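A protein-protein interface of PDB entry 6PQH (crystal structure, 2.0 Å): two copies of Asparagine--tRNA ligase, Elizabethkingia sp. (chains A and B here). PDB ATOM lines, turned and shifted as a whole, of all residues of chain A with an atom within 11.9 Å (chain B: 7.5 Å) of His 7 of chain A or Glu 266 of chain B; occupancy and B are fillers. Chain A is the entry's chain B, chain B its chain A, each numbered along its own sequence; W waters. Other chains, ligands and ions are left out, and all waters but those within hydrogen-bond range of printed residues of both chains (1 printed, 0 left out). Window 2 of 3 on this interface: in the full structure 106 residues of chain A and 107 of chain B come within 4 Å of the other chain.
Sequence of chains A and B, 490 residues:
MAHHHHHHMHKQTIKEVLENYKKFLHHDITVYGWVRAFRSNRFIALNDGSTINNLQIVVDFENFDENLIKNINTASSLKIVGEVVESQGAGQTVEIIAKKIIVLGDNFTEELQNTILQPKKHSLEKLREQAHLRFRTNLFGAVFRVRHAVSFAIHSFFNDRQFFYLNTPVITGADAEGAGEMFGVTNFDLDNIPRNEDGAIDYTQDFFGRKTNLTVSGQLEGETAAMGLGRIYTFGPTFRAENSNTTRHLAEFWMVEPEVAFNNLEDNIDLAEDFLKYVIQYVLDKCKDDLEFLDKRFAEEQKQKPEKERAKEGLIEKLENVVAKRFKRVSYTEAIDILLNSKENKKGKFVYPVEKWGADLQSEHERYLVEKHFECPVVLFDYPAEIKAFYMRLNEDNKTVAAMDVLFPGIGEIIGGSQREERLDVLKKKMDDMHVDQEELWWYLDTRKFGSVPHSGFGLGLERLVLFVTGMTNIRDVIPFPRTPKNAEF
Water W1 lies within hydrogen-bond range of OD2 of Asp 267 of chain B (2.5 Å) and NZ of Lys 11 of chain A (3.2 Å).
Along chain A the printed residues that touch a printed residue of chain B span positions 7 to 11.
Of the 16 printed residues of chain B, 4 touch a printed residue of chain A.
The backbone carbonyl oxygen (O) of Asn 263 of chain B sits at hydrogen-bond distance from the side-chain hydroxyl (OG) of Ser 456 of chain B (2.7 Å).
OD1 of Asn 264 of chain B lies within hydrogen-bond range of N of Glu 266 of chain B, at 3.1 Å.
N of Asp 267 of chain B is in hydrogen-bond range of OD1 of Asn 264 of chain B, 2.8 Å away.
The side-chain carboxylate (OD1) of Asp 270 of chain B lies within salt-bridge range of the guanidinium group (NH2) of Arg 329 of chain B, at 2.7 Å.
The side-chain carboxylate (OD2) of Asp 267 of chain B lies within salt-bridge range of the side-chain amino group (NZ) of Lys 11 of chain A, 3.1 Å away.
O of His 7 of chain A sits close to OE2 of Glu 266 of chain B, at 3.2 Å.
No position is printed for both chains.
Among the printed residues, merely in contact across the chains: His 8 of chain A with Glu 266 of chain B, His 8 of chain A with Asp 270 of chain B and Lys 11 of chain A with Asn 263 of chain B.
Printed residues of chain B within 4 Å of His 8 of chain A: Glu 266 and Asp 270.
Printed residues of chain B within 4 Å of Lys 11 of chain A: Asn 263 and Asp 267.
Printed residues of chain A within 4 Å of Asn 263 of chain B: Lys 11.
Asn 264 of chain B touches none of the printed residues of chain A.
No residue of chain A comes within 4 Å of Leu 265 of chain B.
Glu 266 of chain B touches just these residues of chain A: His 7 (3.2 Å) and His 8 (3.7 Å).
Asp 267 of chain B touches one residue of chain A.
Asn 268 of chain B touches none of the printed residues of chain A.
No residue of chain A comes within 4 Å of Ile 269 of chain B.
Printed residues of chain A within 4 Å of Asp 270 of chain B: His 8.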
ATOM      1  N   HIS A   7      -1.684   4.742  -8.690  1.00  0.00           N
ATOM      2  CA  HIS A   7      -1.637   6.076  -9.270  1.00  0.00           C
ATOM      3  C   HIS A   7      -1.143   6.023 -10.713  1.00  0.00           C
ATOM      4  O   HIS A   7      -0.438   6.927 -11.165  1.00  0.00           O
ATOM      5  CB  HIS A   7      -0.739   6.994  -8.440  1.00  0.00           C
ATOM      6  N   HIS A   8      -1.510   4.956 -11.426  1.00  0.00           N
ATOM      7  CA  HIS A   8      -1.199   4.828 -12.846  1.00  0.00           C
ATOM      8  C   HIS A   8      -2.114   3.775 -13.454  1.00  0.00           C
ATOM      9  O   HIS A   8      -2.181   2.645 -12.956  1.00  0.00           O
ATOM     10  CB  HIS A   8       0.269   4.456 -13.074  1.00  0.00           C
ATOM     11  N   MET A   9      -2.805   4.147 -14.530  1.00  0.00           N
ATOM     12  CA  MET A   9      -3.810   3.274 -15.122  1.00  0.00           C
ATOM     13  C   MET A   9      -3.179   2.005 -15.687  1.00  0.00           C
ATOM     14  O   MET A   9      -2.079   2.025 -16.246  1.00  0.00           O
ATOM     15  CB  MET A   9      -4.577   4.011 -16.225  1.00  0.00           C
ATOM     16  N   HIS A  10      -3.889   0.898 -15.525  1.00  0.00           N
ATOM     17  CA  HIS A  10      -3.459  -0.372 -16.084  1.00  0.00           C
ATOM     18  C   HIS A  10      -3.631  -0.359 -17.601  1.00  0.00           C
ATOM     19  O   HIS A  10      -4.598   0.193 -18.130  1.00  0.00           O
ATOM     20  CB  HIS A  10      -4.271  -1.503 -15.451  1.00  0.00           C
ATOM     21  CG  HIS A  10      -3.955  -2.864 -15.985  1.00  0.00           C
ATOM     22  ND1 HIS A  10      -2.727  -3.466 -15.817  1.00  0.00           N
ATOM     23  CD2 HIS A  10      -4.719  -3.749 -16.667  1.00  0.00           C
ATOM     24  CE1 HIS A  10      -2.744  -4.660 -16.382  1.00  0.00           C
ATOM     25  NE2 HIS A  10      -3.941  -4.856 -16.905  1.00  0.00           N
ATOM     26  N   LYS A  11      -2.674  -0.948 -18.303  1.00  0.00           N
ATOM     27  CA  LYS A  11      -2.773  -1.079 -19.748  1.00  0.00           C
ATOM     28  C   LYS A  11      -3.291  -2.468 -20.106  1.00  0.00           C
ATOM     29  O   LYS A  11      -3.165  -3.415 -19.328  1.00  0.00           O
ATOM     30  CB  LYS A  11      -1.422  -0.818 -20.414  1.00  0.00           C
ATOM     31  CG  LYS A  11      -0.859   0.578 -20.151  1.00  0.00           C
ATOM     32  CD  LYS A  11       0.333   0.844 -21.073  1.00  0.00           C
ATOM     33  CE  LYS A  11       0.942   2.216 -20.842  1.00  0.00           C
ATOM     34  NZ  LYS A  11       1.351   2.423 -19.427  1.00  0.00           N
ATOM     35  N   TYR A  32      -2.742   1.482 -27.349  1.00  0.00           N
ATOM     36  CA  TYR A  32      -1.505   1.974 -27.940  1.00  0.00           C
ATOM     37  C   TYR A  32      -1.074   1.031 -29.057  1.00  0.00           C
ATOM     38  O   TYR A  32      -1.215  -0.189 -28.935  1.00  0.00           O
ATOM     39  CB  TYR A  32      -0.365   2.048 -26.886  1.00  0.00           C
ATOM     40  CG  TYR A  32      -0.642   2.878 -25.654  1.00  0.00           C
ATOM     41  CD1 TYR A  32      -0.127   4.160 -25.531  1.00  0.00           C
ATOM     42  CD2 TYR A  32      -1.392   2.371 -24.600  1.00  0.00           C
ATOM     43  CE1 TYR A  32      -0.371   4.929 -24.394  1.00  0.00           C
ATOM     44  CE2 TYR A  32      -1.635   3.131 -23.459  1.00  0.00           C
ATOM     45  CZ  TYR A  32      -1.122   4.409 -23.368  1.00  0.00           C
ATOM     46  OH  TYR A  32      -1.367   5.171 -22.254  1.00  0.00           O
ATOM     47  N   ASN B 263       5.709   2.330 -22.044  1.00  0.00           N
ATOM     48  CA  ASN B 263       5.993   2.578 -20.634  1.00  0.00           C
ATOM     49  C   ASN B 263       6.855   3.823 -20.473  1.00  0.00           C
ATOM     50  O   ASN B 263       7.851   3.988 -21.180  1.00  0.00           O
ATOM     51  CB  ASN B 263       6.704   1.378 -20.012  1.00  0.00           C
ATOM     52  CG  ASN B 263       5.738   0.346 -19.479  1.00  0.00           C
ATOM     53  OD1 ASN B 263       4.538   0.436 -19.723  1.00  0.00           O
ATOM     54  ND2 ASN B 263       6.254  -0.640 -18.744  1.00  0.00           N
ATOM     55  N   ASN B 264       6.474   4.692 -19.548  1.00  0.00           N
ATOM     56  CA  ASN B 264       7.323   5.799 -19.125  1.00  0.00           C
ATOM     57  C   ASN B 264       8.117   5.382 -17.882  1.00  0.00           C
ATOM     58  O   ASN B 264       8.080   4.225 -17.458  1.00  0.00           O
ATOM     59  CB  ASN B 264       6.479   7.053 -18.869  1.00  0.00           C
ATOM     60  CG  ASN B 264       5.489   6.885 -17.705  1.00  0.00           C
ATOM     61  OD1 ASN B 264       5.572   5.948 -16.921  1.00  0.00           O
ATOM     62  ND2 ASN B 264       4.555   7.813 -17.597  1.00  0.00           N
ATOM     63  N   LEU B 265       8.804   6.332 -17.243  1.00  0.00           N
ATOM     64  CA  LEU B 265       9.667   5.966 -16.116  1.00  0.00           C
ATOM     65  C   LEU B 265       8.854   5.391 -14.961  1.00  0.00           C
ATOM     66  O   LEU B 265       9.216   4.359 -14.383  1.00  0.00           O
ATOM     67  CB  LEU B 265      10.488   7.169 -15.648  1.00  0.00           C
ATOM     68  CG  LEU B 265      11.353   6.869 -14.403  1.00  0.00           C
ATOM     69  CD1 LEU B 265      12.282   5.677 -14.634  1.00  0.00           C
ATOM     70  CD2 LEU B 265      12.144   8.106 -13.910  1.00  0.00           C
ATOM     71  N   GLU B 266       7.729   6.032 -14.629  1.00  0.00           N
ATOM     72  CA  GLU B 266       6.899   5.538 -13.534  1.00  0.00           C
ATOM     73  C   GLU B 266       6.402   4.118 -13.805  1.00  0.00           C
ATOM     74  O   GLU B 266       6.414   3.269 -12.902  1.00  0.00           O
ATOM     75  CB  GLU B 266       5.717   6.480 -13.302  1.00  0.00           C
ATOM     76  CG  GLU B 266       4.796   5.986 -12.199  1.00  0.00           C
ATOM     77  CD  GLU B 266       3.666   6.948 -11.911  1.00  0.00           C
ATOM     78  OE1 GLU B 266       3.745   8.103 -12.372  1.00  0.00           O
ATOM     79  OE2 GLU B 266       2.701   6.541 -11.236  1.00  0.00           O
ATOM     80  N   ASP B 267       5.960   3.845 -15.041  1.00  0.00           N
ATOM     81  CA  ASP B 267       5.579   2.487 -15.423  1.00  0.00           C
ATOM     82  C   ASP B 267       6.745   1.522 -15.257  1.00  0.00           C
ATOM     83  O   ASP B 267       6.569   0.367 -14.844  1.00  0.00           O
ATOM     84  CB  ASP B 267       5.135   2.459 -16.888  1.00  0.00           C
ATOM     85  CG  ASP B 267       3.911   3.286 -17.158  1.00  0.00           C
ATOM     86  OD1 ASP B 267       2.993   3.312 -16.304  1.00  0.00           O
ATOM     87  OD2 ASP B 267       3.859   3.881 -18.260  1.00  0.00           O
ATOM     88  N   ASN B 268       7.937   1.969 -15.640  1.00  0.00           N
ATOM     89  CA  ASN B 268       9.135   1.151 -15.510  1.00  0.00           C
ATOM     90  C   ASN B 268       9.384   0.779 -14.055  1.00  0.00           C
ATOM     91  O   ASN B 268       9.752  -0.361 -13.755  1.00  0.00           O
ATOM     92  CB  ASN B 268      10.333   1.920 -16.095  1.00  0.00           C
ATOM     93  CG  ASN B 268      11.475   1.014 -16.531  1.00  0.00           C
ATOM     94  OD1 ASN B 268      11.258  -0.078 -17.045  1.00  0.00           O
ATOM     95  ND2 ASN B 268      12.709   1.487 -16.340  1.00  0.00           N
ATOM     96  N   ILE B 269       9.192   1.729 -13.130  1.00  0.00           N
ATOM     97  CA  ILE B 269       9.423   1.422 -11.722  1.00  0.00           C
ATOM     98  C   ILE B 269       8.353   0.469 -11.208  1.00  0.00           C
ATOM     99  O   ILE B 269       8.653  -0.491 -10.487  1.00  0.00           O
ATOM    100  CB  ILE B 269       9.477   2.715 -10.892  1.00  0.00           C
ATOM    101  CG1 ILE B 269      10.673   3.569 -11.316  1.00  0.00           C
ATOM    102  CG2 ILE B 269       9.564   2.392  -9.398  1.00  0.00           C
ATOM    103  CD1 ILE B 269      10.589   5.018 -10.798  1.00  0.00           C
ATOM    104  N   ASP B 270       7.091   0.714 -11.573  1.00  0.00           N
ATOM    105  CA  ASP B 270       6.020  -0.228 -11.244  1.00  0.00           C
ATOM    106  C   ASP B 270       6.371  -1.635 -11.698  1.00  0.00           C
ATOM    107  O   ASP B 270       6.220  -2.602 -10.945  1.00  0.00           O
ATOM    108  CB  ASP B 270       4.713   0.198 -11.915  1.00  0.00           C
ATOM    109  CG  ASP B 270       4.167   1.500 -11.370  1.00  0.00           C
ATOM    110  OD1 ASP B 270       4.659   1.998 -10.331  1.00  0.00           O
ATOM    111  OD2 ASP B 270       3.246   2.029 -12.009  1.00  0.00           O
ATOM    112  N   LEU B 271       6.806  -1.765 -12.954  1.00  0.00           N
ATOM    113  CA  LEU B 271       7.173  -3.070 -13.490  1.00  0.00           C
ATOM    114  C   LEU B 271       8.290  -3.706 -12.670  1.00  0.00           C
ATOM    115  O   LEU B 271       8.214  -4.882 -12.301  1.00  0.00           O
ATOM    116  CB  LEU B 271       7.588  -2.926 -14.960  1.00  0.00           C
ATOM    117  CG  LEU B 271       7.996  -4.210 -15.655  1.00  0.00           C
ATOM    118  CD1 LEU B 271       6.838  -5.201 -15.651  1.00  0.00           C
ATOM    119  CD2 LEU B 271       8.473  -3.921 -17.062  1.00  0.00           C
ATOM    120  N   ALA B 272       9.339  -2.944 -12.366  1.00  0.00           N
ATOM    121  CA  ALA B 272      10.448  -3.504 -11.589  1.00  0.00           C
ATOM    122  C   ALA B 272       9.973  -3.996 -10.222  1.00  0.00           C
ATOM    123  O   ALA B 272      10.346  -5.091  -9.774  1.00  0.00           O
ATOM    124  CB  ALA B 272      11.552  -2.456 -11.427  1.00  0.00           C
ATOM    125  N   ARG B 326       5.911  -1.537   0.352  1.00  0.00           N
ATOM    126  CA  ARG B 326       5.960  -0.717  -0.855  1.00  0.00           C
ATOM    127  C   ARG B 326       7.327  -0.050  -0.954  1.00  0.00           C
ATOM    128  O   ARG B 326       7.818   0.505   0.029  1.00  0.00           O
ATOM    129  CB  ARG B 326       4.862   0.353  -0.835  1.00  0.00           C
ATOM    130  CG  ARG B 326       3.447  -0.165  -1.091  1.00  0.00           C
ATOM    131  CD  ARG B 326       3.379  -1.168  -2.251  1.00  0.00           C
ATOM    132  NE  ARG B 326       3.799  -0.616  -3.540  1.00  0.00           N
ATOM    133  CZ  ARG B 326       3.020   0.110  -4.337  1.00  0.00           C
ATOM    134  NH1 ARG B 326       1.775   0.394  -3.977  1.00  0.00           N
ATOM    135  NH2 ARG B 326       3.488   0.561  -5.494  1.00  0.00           N
ATOM    136  N   ARG B 329      10.067   5.620  -3.198  1.00  0.00           N
ATOM    137  CA  ARG B 329      10.538   6.249  -4.429  1.00  0.00           C
ATOM    138  C   ARG B 329      11.040   7.644  -4.090  1.00  0.00           C
ATOM    139  O   ARG B 329      10.263   8.487  -3.619  1.00  0.00           O
ATOM    140  CB  ARG B 329       9.436   6.286  -5.490  1.00  0.00           C
ATOM    141  CG  ARG B 329       8.879   4.910  -5.774  1.00  0.00           C
ATOM    142  CD  ARG B 329       7.786   4.914  -6.852  1.00  0.00           C
ATOM    143  NE  ARG B 329       7.211   3.576  -7.000  1.00  0.00           N
ATOM    144  CZ  ARG B 329       6.572   3.144  -8.081  1.00  0.00           C
ATOM    145  NH1 ARG B 329       6.418   3.927  -9.145  1.00  0.00           N
ATOM    146  NH2 ARG B 329       6.096   1.910  -8.104  1.00  0.00           N
ATOM    147  N   ALA B 402      15.835  10.460 -17.026  1.00  0.00           N
ATOM    148  CA  ALA B 402      14.828   9.566 -16.453  1.00  0.00           C
ATOM    149  C   ALA B 402      15.422   8.193 -16.133  1.00  0.00           C
ATOM    150  O   ALA B 402      14.973   7.159 -16.616  1.00  0.00           O
ATOM    151  CB  ALA B 402      13.638   9.441 -17.398  1.00  0.00           C
ATOM    152  N   MET B 404      16.545   5.190 -13.243  1.00  0.00           N
ATOM    153  CA  MET B 404      16.095   4.649 -11.971  1.00  0.00           C
ATOM    154  C   MET B 404      17.028   3.530 -11.536  1.00  0.00           C
ATOM    155  O   MET B 404      17.587   2.806 -12.369  1.00  0.00           O
ATOM    156  CB  MET B 404      14.640   4.154 -12.044  1.00  0.00           C
ATOM    157  CG  MET B 404      14.365   3.085 -13.067  1.00  0.00           C
ATOM    158  SD  MET B 404      14.542   1.411 -12.424  1.00  0.00           S
ATOM    159  CE  MET B 404      12.934   0.733 -12.791  1.00  0.00           C
ATOM    160  N   GLN B 419      13.747   5.327 -18.575  1.00  0.00           N
ATOM    161  CA  GLN B 419      12.974   5.626 -19.767  1.00  0.00           C
ATOM    162  C   GLN B 419      13.943   6.087 -20.842  1.00  0.00           C
ATOM    163  O   GLN B 419      14.886   6.827 -20.552  1.00  0.00           O
ATOM    164  CB  GLN B 419      11.923   6.704 -19.487  1.00  0.00           C
ATOM    165  CG  GLN B 419      11.087   7.065 -20.738  1.00  0.00           C
ATOM    166  CD  GLN B 419       9.876   7.909 -20.405  1.00  0.00           C
ATOM    167  OE1 GLN B 419       9.599   8.191 -19.226  1.00  0.00           O
ATOM    168  NE2 GLN B 419       9.131   8.306 -21.443  1.00  0.00           N
ATOM    169  N   SER B 456      10.605   2.255 -22.151  1.00  0.00           N
ATOM    170  CA  SER B 456      11.435   2.133 -20.958  1.00  0.00           C
ATOM    171  C   SER B 456      11.779   0.674 -20.729  1.00  0.00           C
ATOM    172  O   SER B 456      10.994  -0.218 -21.068  1.00  0.00           O
ATOM    173  CB  SER B 456      10.716   2.641 -19.696  1.00  0.00           C
ATOM    174  OG  SER B 456      10.184   3.936 -19.875  1.00  0.00           O
HETATM  175  O   HOH W   1       2.312   5.429 -19.518  1.00  0.00           O
